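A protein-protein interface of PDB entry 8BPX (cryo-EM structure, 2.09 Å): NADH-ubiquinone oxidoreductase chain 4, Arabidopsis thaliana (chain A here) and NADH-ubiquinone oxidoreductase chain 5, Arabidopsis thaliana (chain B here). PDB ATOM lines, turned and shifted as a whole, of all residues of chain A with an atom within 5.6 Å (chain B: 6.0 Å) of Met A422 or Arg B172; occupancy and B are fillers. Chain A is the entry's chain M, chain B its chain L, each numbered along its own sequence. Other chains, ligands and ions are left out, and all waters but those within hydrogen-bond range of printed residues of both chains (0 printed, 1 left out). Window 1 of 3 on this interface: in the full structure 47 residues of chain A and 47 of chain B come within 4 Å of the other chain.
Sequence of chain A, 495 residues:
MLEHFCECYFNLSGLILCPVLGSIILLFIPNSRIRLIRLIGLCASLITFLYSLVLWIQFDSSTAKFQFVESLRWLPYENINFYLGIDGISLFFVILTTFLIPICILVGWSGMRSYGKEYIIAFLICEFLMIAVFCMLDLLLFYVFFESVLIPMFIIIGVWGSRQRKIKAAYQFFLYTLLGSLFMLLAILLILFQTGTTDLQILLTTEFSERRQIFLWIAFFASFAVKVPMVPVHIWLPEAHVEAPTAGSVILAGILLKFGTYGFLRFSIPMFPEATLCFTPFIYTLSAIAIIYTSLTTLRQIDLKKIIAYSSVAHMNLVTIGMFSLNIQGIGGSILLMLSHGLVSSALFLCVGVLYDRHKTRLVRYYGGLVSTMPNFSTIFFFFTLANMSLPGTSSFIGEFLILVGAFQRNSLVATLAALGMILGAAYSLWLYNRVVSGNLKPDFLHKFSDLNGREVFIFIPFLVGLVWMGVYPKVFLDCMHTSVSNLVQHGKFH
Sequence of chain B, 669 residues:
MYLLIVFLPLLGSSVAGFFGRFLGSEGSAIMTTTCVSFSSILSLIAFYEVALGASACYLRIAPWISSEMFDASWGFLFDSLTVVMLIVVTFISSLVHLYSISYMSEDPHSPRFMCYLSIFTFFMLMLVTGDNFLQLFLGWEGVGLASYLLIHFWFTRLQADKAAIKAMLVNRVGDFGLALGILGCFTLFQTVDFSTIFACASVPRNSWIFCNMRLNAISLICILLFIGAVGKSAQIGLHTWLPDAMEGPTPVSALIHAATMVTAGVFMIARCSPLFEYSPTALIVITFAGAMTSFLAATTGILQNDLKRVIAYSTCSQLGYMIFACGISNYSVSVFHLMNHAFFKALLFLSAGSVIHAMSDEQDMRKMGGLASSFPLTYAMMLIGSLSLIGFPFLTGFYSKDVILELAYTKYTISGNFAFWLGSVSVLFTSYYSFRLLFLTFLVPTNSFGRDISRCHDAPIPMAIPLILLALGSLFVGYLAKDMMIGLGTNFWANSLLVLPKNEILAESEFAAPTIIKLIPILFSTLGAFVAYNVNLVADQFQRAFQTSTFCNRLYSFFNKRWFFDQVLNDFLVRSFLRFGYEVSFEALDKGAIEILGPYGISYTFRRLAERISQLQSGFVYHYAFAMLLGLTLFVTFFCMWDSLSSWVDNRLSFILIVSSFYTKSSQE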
ATOM      1  N   MET A 389     -15.755 -24.098  19.855  1.00  0.00           N
ATOM      2  CA  MET A 389     -16.122 -22.650  19.962  1.00  0.00           C
ATOM      3  C   MET A 389     -17.115 -22.256  18.839  1.00  0.00           C
ATOM      4  O   MET A 389     -17.356 -21.097  18.704  1.00  0.00           O
ATOM      5  CB  MET A 389     -14.883 -21.743  19.912  1.00  0.00           C
ATOM      6  CG  MET A 389     -13.717 -22.046  20.785  1.00  0.00           C
ATOM      7  SD  MET A 389     -12.247 -21.049  20.355  1.00  0.00           S
ATOM      8  CE  MET A 389     -12.986 -19.499  19.848  1.00  0.00           C
ATOM      9  N   SER A 390     -17.553 -23.179  18.009  1.00  0.00           N
ATOM     10  CA  SER A 390     -18.497 -22.927  16.861  1.00  0.00           C
ATOM     11  C   SER A 390     -17.851 -21.988  15.813  1.00  0.00           C
ATOM     12  O   SER A 390     -18.553 -21.137  15.331  1.00  0.00           O
ATOM     13  CB  SER A 390     -19.863 -22.480  17.318  1.00  0.00           C
ATOM     14  OG  SER A 390     -20.593 -23.537  17.886  1.00  0.00           O
ATOM     15  N   LEU A 391     -16.539 -22.041  15.664  1.00  0.00           N
ATOM     16  CA  LEU A 391     -15.824 -21.334  14.589  1.00  0.00           C
ATOM     17  C   LEU A 391     -16.441 -21.604  13.212  1.00  0.00           C
ATOM     18  O   LEU A 391     -16.537 -22.715  12.794  1.00  0.00           O
ATOM     19  CB  LEU A 391     -14.350 -21.711  14.568  1.00  0.00           C
ATOM     20  CG  LEU A 391     -13.506 -20.753  13.729  1.00  0.00           C
ATOM     21  CD1 LEU A 391     -13.235 -19.462  14.477  1.00  0.00           C
ATOM     22  CD2 LEU A 391     -12.223 -21.392  13.227  1.00  0.00           C
ATOM     23  N   PRO A 392     -16.797 -20.565  12.458  1.00  0.00           N
ATOM     24  CA  PRO A 392     -17.301 -20.787  11.096  1.00  0.00           C
ATOM     25  C   PRO A 392     -16.303 -21.576  10.263  1.00  0.00           C
ATOM     26  O   PRO A 392     -15.093 -21.357  10.329  1.00  0.00           O
ATOM     27  CB  PRO A 392     -17.488 -19.366  10.557  1.00  0.00           C
ATOM     28  CG  PRO A 392     -17.731 -18.546  11.775  1.00  0.00           C
ATOM     29  CD  PRO A 392     -16.881 -19.154  12.856  1.00  0.00           C
ATOM     30  N   GLU A 400     -25.294 -24.112  15.351  1.00  0.00           N
ATOM     31  CA  GLU A 400     -25.407 -23.010  16.299  1.00  0.00           C
ATOM     32  C   GLU A 400     -26.102 -21.807  15.674  1.00  0.00           C
ATOM     33  O   GLU A 400     -27.043 -21.242  16.251  1.00  0.00           O
ATOM     34  CB  GLU A 400     -24.024 -22.630  16.818  1.00  0.00           C
ATOM     35  CG  GLU A 400     -24.055 -21.719  18.014  1.00  0.00           C
ATOM     36  CD  GLU A 400     -23.336 -20.412  17.764  1.00  0.00           C
ATOM     37  OE1 GLU A 400     -22.937 -20.158  16.609  1.00  0.00           O
ATOM     38  OE2 GLU A 400     -23.172 -19.635  18.724  1.00  0.00           O
ATOM     39  N   LEU A 404     -29.792 -20.088  16.372  1.00  0.00           N
ATOM     40  CA  LEU A 404     -29.977 -18.676  16.695  1.00  0.00           C
ATOM     41  C   LEU A 404     -30.957 -18.014  15.723  1.00  0.00           C
ATOM     42  O   LEU A 404     -31.778 -17.186  16.133  1.00  0.00           O
ATOM     43  CB  LEU A 404     -28.632 -17.951  16.709  1.00  0.00           C
ATOM     44  CG  LEU A 404     -27.653 -18.337  17.824  1.00  0.00           C
ATOM     45  CD1 LEU A 404     -26.318 -17.629  17.667  1.00  0.00           C
ATOM     46  CD2 LEU A 404     -28.238 -18.070  19.208  1.00  0.00           C
ATOM     47  N   ALA A 418     -28.940 -16.698  24.375  1.00  0.00           N
ATOM     48  CA  ALA A 418     -28.270 -17.858  23.734  1.00  0.00           C
ATOM     49  C   ALA A 418     -27.008 -17.471  22.946  1.00  0.00           C
ATOM     50  O   ALA A 418     -26.078 -18.196  23.024  1.00  0.00           O
ATOM     51  CB  ALA A 418     -29.240 -18.658  22.929  1.00  0.00           C
ATOM     52  N   ALA A 419     -26.969 -16.296  22.333  1.00  0.00           N
ATOM     53  CA  ALA A 419     -25.763 -15.836  21.627  1.00  0.00           C
ATOM     54  C   ALA A 419     -24.604 -15.483  22.622  1.00  0.00           C
ATOM     55  O   ALA A 419     -23.517 -15.464  22.166  1.00  0.00           O
ATOM     56  CB  ALA A 419     -26.133 -14.759  20.653  1.00  0.00           C
ATOM     57  N   LEU A 420     -24.877 -15.199  23.902  1.00  0.00           N
ATOM     58  CA  LEU A 420     -23.809 -15.044  24.960  1.00  0.00           C
ATOM     59  C   LEU A 420     -22.881 -16.261  25.010  1.00  0.00           C
ATOM     60  O   LEU A 420     -21.719 -16.047  25.275  1.00  0.00           O
ATOM     61  CB  LEU A 420     -24.399 -14.765  26.342  1.00  0.00           C
ATOM     62  CG  LEU A 420     -25.127 -13.429  26.453  1.00  0.00           C
ATOM     63  CD1 LEU A 420     -25.857 -13.300  27.777  1.00  0.00           C
ATOM     64  CD2 LEU A 420     -24.182 -12.265  26.221  1.00  0.00           C
ATOM     65  N   GLY A 421     -23.379 -17.464  24.708  1.00  0.00           N
ATOM     66  CA  GLY A 421     -22.550 -18.669  24.574  1.00  0.00           C
ATOM     67  C   GLY A 421     -21.346 -18.500  23.662  1.00  0.00           C
ATOM     68  O   GLY A 421     -20.316 -19.048  24.014  1.00  0.00           O
ATOM     69  N   MET A 422     -21.467 -17.790  22.547  1.00  0.00           N
ATOM     70  CA  MET A 422     -20.322 -17.442  21.684  1.00  0.00           C
ATOM     71  C   MET A 422     -19.196 -16.820  22.526  1.00  0.00           C
ATOM     72  O   MET A 422     -18.069 -17.108  22.256  1.00  0.00           O
ATOM     73  CB  MET A 422     -20.713 -16.510  20.527  1.00  0.00           C
ATOM     74  CG  MET A 422     -21.966 -16.865  19.743  1.00  0.00           C
ATOM     75  SD  MET A 422     -22.634 -15.414  18.814  1.00  0.00           S
ATOM     76  CE  MET A 422     -21.199 -14.942  17.853  1.00  0.00           C
ATOM     77  N   ILE A 423     -19.493 -15.979  23.470  1.00  0.00           N
ATOM     78  CA  ILE A 423     -18.429 -15.322  24.257  1.00  0.00           C
ATOM     79  C   ILE A 423     -17.879 -16.288  25.346  1.00  0.00           C
ATOM     80  O   ILE A 423     -16.696 -16.402  25.464  1.00  0.00           O
ATOM     81  CB  ILE A 423     -18.884 -13.953  24.825  1.00  0.00           C
ATOM     82  CG1 ILE A 423     -19.384 -13.002  23.732  1.00  0.00           C
ATOM     83  CG2 ILE A 423     -17.807 -13.318  25.690  1.00  0.00           C
ATOM     84  CD1 ILE A 423     -20.298 -11.908  24.235  1.00  0.00           C
ATOM     85  N   LEU A 424     -18.756 -16.974  26.044  1.00  0.00           N
ATOM     86  CA  LEU A 424     -18.320 -17.779  27.188  1.00  0.00           C
ATOM     87  C   LEU A 424     -17.614 -19.067  26.751  1.00  0.00           C
ATOM     88  O   LEU A 424     -16.583 -19.448  27.329  1.00  0.00           O
ATOM     89  CB  LEU A 424     -19.514 -18.070  28.092  1.00  0.00           C
ATOM     90  CG  LEU A 424     -20.185 -16.828  28.692  1.00  0.00           C
ATOM     91  CD1 LEU A 424     -21.426 -17.196  29.482  1.00  0.00           C
ATOM     92  CD2 LEU A 424     -19.214 -16.038  29.561  1.00  0.00           C
ATOM     93  N   GLY A 425     -18.156 -19.752  25.739  1.00  0.00           N
ATOM     94  CA  GLY A 425     -17.520 -20.958  25.242  1.00  0.00           C
ATOM     95  C   GLY A 425     -16.138 -20.699  24.681  1.00  0.00           C
ATOM     96  O   GLY A 425     -15.209 -21.474  24.916  1.00  0.00           O
ATOM     97  N   ALA A 426     -15.959 -19.562  23.956  1.00  0.00           N
ATOM     98  CA  ALA A 426     -14.622 -19.148  23.499  1.00  0.00           C
ATOM     99  C   ALA A 426     -13.707 -19.017  24.717  1.00  0.00           C
ATOM    100  O   ALA A 426     -12.617 -19.488  24.666  1.00  0.00           O
ATOM    101  CB  ALA A 426     -14.593 -17.850  22.702  1.00  0.00           C
ATOM    102  N   ALA A 427     -14.191 -18.312  25.694  1.00  0.00           N
ATOM    103  CA  ALA A 427     -13.334 -18.053  26.844  1.00  0.00           C
ATOM    104  C   ALA A 427     -12.795 -19.354  27.435  1.00  0.00           C
ATOM    105  O   ALA A 427     -11.575 -19.535  27.556  1.00  0.00           O
ATOM    106  CB  ALA A 427     -14.095 -17.249  27.897  1.00  0.00           C
ATOM    107  N   PHE B 137     -19.015 -13.046   7.758  1.00  0.00           N
ATOM    108  CA  PHE B 137     -18.814 -13.501   9.129  1.00  0.00           C
ATOM    109  C   PHE B 137     -17.705 -14.544   9.205  1.00  0.00           C
ATOM    110  O   PHE B 137     -16.913 -14.556  10.154  1.00  0.00           O
ATOM    111  CB  PHE B 137     -20.127 -14.052   9.683  1.00  0.00           C
ATOM    112  CG  PHE B 137     -20.118 -14.278  11.160  1.00  0.00           C
ATOM    113  CD1 PHE B 137     -20.306 -13.226  12.035  1.00  0.00           C
ATOM    114  CD2 PHE B 137     -19.932 -15.548  11.677  1.00  0.00           C
ATOM    115  CE1 PHE B 137     -20.303 -13.434  13.400  1.00  0.00           C
ATOM    116  CE2 PHE B 137     -19.927 -15.761  13.041  1.00  0.00           C
ATOM    117  CZ  PHE B 137     -20.116 -14.703  13.902  1.00  0.00           C
ATOM    118  N   GLU B 141     -14.409 -14.036  11.560  1.00  0.00           N
ATOM    119  CA  GLU B 141     -13.894 -14.994  12.577  1.00  0.00           C
ATOM    120  C   GLU B 141     -12.507 -15.503  12.161  1.00  0.00           C
ATOM    121  O   GLU B 141     -11.670 -15.699  13.060  1.00  0.00           O
ATOM    122  CB  GLU B 141     -14.869 -16.155  12.763  1.00  0.00           C
ATOM    123  CG  GLU B 141     -16.295 -15.697  12.990  1.00  0.00           C
ATOM    124  CD  GLU B 141     -16.500 -14.718  14.127  1.00  0.00           C
ATOM    125  OE1 GLU B 141     -16.351 -15.132  15.294  1.00  0.00           O
ATOM    126  OE2 GLU B 141     -16.814 -13.547  13.838  1.00  0.00           O
ATOM    127  N   ALA B 167      -7.486 -10.288  23.031  1.00  0.00           N
ATOM    128  CA  ALA B 167      -7.921  -9.893  21.694  1.00  0.00           C
ATOM    129  C   ALA B 167      -9.066 -10.775  21.215  1.00  0.00           C
ATOM    130  O   ALA B 167     -10.084 -10.276  20.715  1.00  0.00           O
ATOM    131  CB  ALA B 167      -6.745  -9.954  20.721  1.00  0.00           C
ATOM    132  N   MET B 168      -8.901 -12.101  21.282  1.00  0.00           N
ATOM    133  CA  MET B 168     -10.029 -13.010  20.926  1.00  0.00           C
ATOM    134  C   MET B 168     -11.342 -12.718  21.673  1.00  0.00           C
ATOM    135  O   MET B 168     -12.343 -12.696  21.015  1.00  0.00           O
ATOM    136  CB  MET B 168      -9.678 -14.496  21.043  1.00  0.00           C
ATOM    137  CG  MET B 168      -8.970 -15.052  19.852  1.00  0.00           C
ATOM    138  SD  MET B 168     -10.066 -15.676  18.560  1.00  0.00           S
ATOM    139  CE  MET B 168     -11.572 -15.895  19.502  1.00  0.00           C
ATOM    140  N   LEU B 169     -11.314 -12.516  22.976  1.00  0.00           N
ATOM    141  CA  LEU B 169     -12.538 -12.270  23.775  1.00  0.00           C
ATOM    142  C   LEU B 169     -13.208 -10.917  23.428  1.00  0.00           C
ATOM    143  O   LEU B 169     -14.390 -10.887  23.336  1.00  0.00           O
ATOM    144  CB  LEU B 169     -12.193 -12.332  25.259  1.00  0.00           C
ATOM    145  CG  LEU B 169     -11.730 -13.697  25.783  1.00  0.00           C
ATOM    146  CD1 LEU B 169     -11.268 -13.642  27.232  1.00  0.00           C
ATOM    147  CD2 LEU B 169     -12.806 -14.751  25.610  1.00  0.00           C
ATOM    148  N   VAL B 170     -12.433  -9.855  23.281  1.00  0.00           N
ATOM    149  CA  VAL B 170     -13.007  -8.541  22.849  1.00  0.00           C
ATOM    150  C   VAL B 170     -13.643  -8.698  21.463  1.00  0.00           C
ATOM    151  O   VAL B 170     -14.767  -8.305  21.341  1.00  0.00           O
ATOM    152  CB  VAL B 170     -12.005  -7.369  22.980  1.00  0.00           C
ATOM    153  CG1 VAL B 170     -12.659  -6.046  22.653  1.00  0.00           C
ATOM    154  CG2 VAL B 170     -11.392  -7.294  24.370  1.00  0.00           C
ATOM    155  N   ASN B 171     -12.974  -9.380  20.550  1.00  0.00           N
ATOM    156  CA  ASN B 171     -13.490  -9.594  19.178  1.00  0.00           C
ATOM    157  C   ASN B 171     -14.766 -10.443  19.215  1.00  0.00           C
ATOM    158  O   ASN B 171     -15.661 -10.091  18.522  1.00  0.00           O
ATOM    159  CB  ASN B 171     -12.374  -9.984  18.203  1.00  0.00           C
ATOM    160  CG  ASN B 171     -11.608  -8.728  17.807  1.00  0.00           C
ATOM    161  OD1 ASN B 171     -12.121  -7.890  17.068  1.00  0.00           O
ATOM    162  ND2 ASN B 171     -10.415  -8.524  18.349  1.00  0.00           N
ATOM    163  N   ARG B 172     -14.826 -11.455  20.100  1.00  0.00           N
ATOM    164  CA  ARG B 172     -16.054 -12.262  20.275  1.00  0.00           C
ATOM    165  C   ARG B 172     -17.220 -11.365  20.746  1.00  0.00           C
ATOM    166  O   ARG B 172     -18.293 -11.620  20.316  1.00  0.00           O
ATOM    167  CB  ARG B 172     -15.804 -13.513  21.141  1.00  0.00           C
ATOM    168  CG  ARG B 172     -15.388 -14.739  20.344  1.00  0.00           C
ATOM    169  CD  ARG B 172     -16.559 -15.388  19.632  1.00  0.00           C
ATOM    170  NE  ARG B 172     -16.178 -16.523  18.813  1.00  0.00           N
ATOM    171  CZ  ARG B 172     -16.497 -17.797  19.036  1.00  0.00           C
ATOM    172  NH1 ARG B 172     -17.222 -18.143  20.081  1.00  0.00           N
ATOM    173  NH2 ARG B 172     -16.076 -18.733  18.208  1.00  0.00           N
ATOM    174  N   VAL B 173     -16.979 -10.406  21.594  1.00  0.00           N
ATOM    175  CA  VAL B 173     -18.054  -9.457  22.039  1.00  0.00           C
ATOM    176  C   VAL B 173     -18.574  -8.660  20.843  1.00  0.00           C
ATOM    177  O   VAL B 173     -19.747  -8.510  20.738  1.00  0.00           O
ATOM    178  CB  VAL B 173     -17.673  -8.589  23.264  1.00  0.00           C
ATOM    179  CG1 VAL B 173     -18.676  -7.484  23.543  1.00  0.00           C
ATOM    180  CG2 VAL B 173     -17.443  -9.419  24.515  1.00  0.00           C
ATOM    181  N   GLY B 174     -17.700  -8.307  19.923  1.00  0.00           N
ATOM    182  CA  GLY B 174     -18.123  -7.659  18.677  1.00  0.00           C
ATOM    183  C   GLY B 174     -18.810  -8.605  17.775  1.00  0.00           C
ATOM    184  O   GLY B 174     -19.820  -8.233  17.242  1.00  0.00           O
ATOM    185  N   ASP B 175     -18.279  -9.822  17.650  1.00  0.00           N
ATOM    186  CA  ASP B 175     -18.907 -10.877  16.824  1.00  0.00           C
ATOM    187  C   ASP B 175     -20.329 -11.167  17.337  1.00  0.00           C
ATOM    188  O   ASP B 175     -21.175 -11.360  16.503  1.00  0.00           O
ATOM    189  CB  ASP B 175     -18.002 -12.104  16.733  1.00  0.00           C
ATOM    190  CG  ASP B 175     -16.569 -11.806  16.345  1.00  0.00           C
ATOM    191  OD1 ASP B 175     -16.319 -10.713  15.814  1.00  0.00           O
ATOM    192  OD2 ASP B 175     -15.710 -12.641  16.637  1.00  0.00           O
ATOM    193  N   PHE B 176     -20.551 -11.111  18.646  1.00  0.00           N
ATOM    194  CA  PHE B 176     -21.894 -11.274  19.243  1.00  0.00           C
ATOM    195  C   PHE B 176     -22.786 -10.189  18.640  1.00  0.00           C
ATOM    196  O   PHE B 176     -23.810 -10.481  18.120  1.00  0.00           O
ATOM    197  CB  PHE B 176     -21.849 -11.184  20.775  1.00  0.00           C
ATOM    198  CG  PHE B 176     -23.109 -10.878  21.528  1.00  0.00           C
ATOM    199  CD1 PHE B 176     -23.968 -11.897  21.903  1.00  0.00           C
ATOM    200  CD2 PHE B 176     -23.387  -9.589  21.948  1.00  0.00           C
ATOM    201  CE1 PHE B 176     -25.109 -11.625  22.633  1.00  0.00           C
ATOM    202  CE2 PHE B 176     -24.527  -9.319  22.684  1.00  0.00           C
ATOM    203  CZ  PHE B 176     -25.383 -10.338  23.026  1.00  0.00           C
ATOM    204  N   GLY B 177     -22.278  -8.972  18.773  1.00  0.00           N
ATOM    205  CA  GLY B 177     -23.079  -7.894  18.205  1.00  0.00           C
ATOM    206  C   GLY B 177     -23.343  -8.081  16.719  1.00  0.00           C
ATOM    207  O   GLY B 177     -24.475  -7.927  16.244  1.00  0.00           O
ATOM    208  N   ALA B 179     -23.331 -10.871  14.909  1.00  0.00           N
ATOM    209  CA  ALA B 179     -24.221 -11.999  14.662  1.00  0.00           C
ATOM    210  C   ALA B 179     -25.669 -11.640  14.965  1.00  0.00           C
ATOM    211  O   ALA B 179     -26.575 -12.033  14.221  1.00  0.00           O
ATOM    212  CB  ALA B 179     -23.780 -13.208  15.487  1.00  0.00           C
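Leu A391 touches none of the printed residues of chain B.
Met A422 touches just these residues of chain B: Arg B172 (2.6 Å), Asp B175 (3.8 Å), Phe B176 (3.97 Å) and Ala B179 (3.9 Å).
Of the printed residues of chain B, Ile A423 touches Arg B172, Val B173 and Phe B176.
Printed residues of chain B within 4 Å of Ala A427: Leu B169 (3.6 Å).
Printed residues of chain A within 4 Å of Phe B137: Pro A392 (3.7 Å).
Of the printed residues of chain A, Leu B169 touches Ala A427 (3.6 Å).
Of the printed residues of chain A, Asp B175 touches Met A422 (3.8 Å).
The nearest residue of chain B that does not touch Met A422 is Phe B137 (4.1 Å).
The nearest residue of chain A that does not touch Arg B172 is Leu A391 (4.2 Å).
The guanidinium group (NE) of Arg B172 lies within salt-bridge range of the side-chain carboxylate (OE1) of Glu B141 (3.8 Å).
O of Met A389 is in hydrogen-bond range of NH2 of Arg B172 (2.7 Å).
The guanidinium group (NH1) of Arg B172 lies within hydrogen-bond range of the backbone carbonyl oxygen (O) of Met A422, at 2.6 Å.
Among the printed residues, pairs that only touch across the chains: Pro A392 with Glu B141 (3.4 Å), Ala A427 with Leu B169 (3.6 Å), Ala A419 with Phe B176 (3.6 Å), Pro A392 with Phe B137 (3.7 Å), Ala A426 with Arg B172 (3.7 Å), Leu A420 with Phe B176 (3.8 Å), Ile A423 with Val B173 (3.8 Å), Met A422 with Asp B175 (3.8 Å), Ile A423 with Arg B172 (3.8 Å), Ile A423 with Phe B176 (3.9 Å), Met A389 with Met B168 (3.9 Å), Met A422 with Ala B179 (3.9 Å) and Met A422 with Phe B176 (3.97 Å).
Of the 14 printed residues of chain B, 9 touch a printed residue of chain A.
Hydrophobic or aromatic side chains of chain B within 4 Å of the printed part of chain A: Phe B137, Met B168, Leu B169, Val B173, Phe B176 and Ala B179.
Printed residues of chain A that touch a printed residue of chain B: Met A389, Pro A392, Ala A419, Leu A420, Met A422, Ile A423, Ala A426 and Ala A427.
Hydrophobic or aromatic side chains of chain A that line the printed part of chain B: Met A389, Pro A392, Ala A419, Leu A420, Met A422, Ile A423, Ala A426 and Ala A427.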
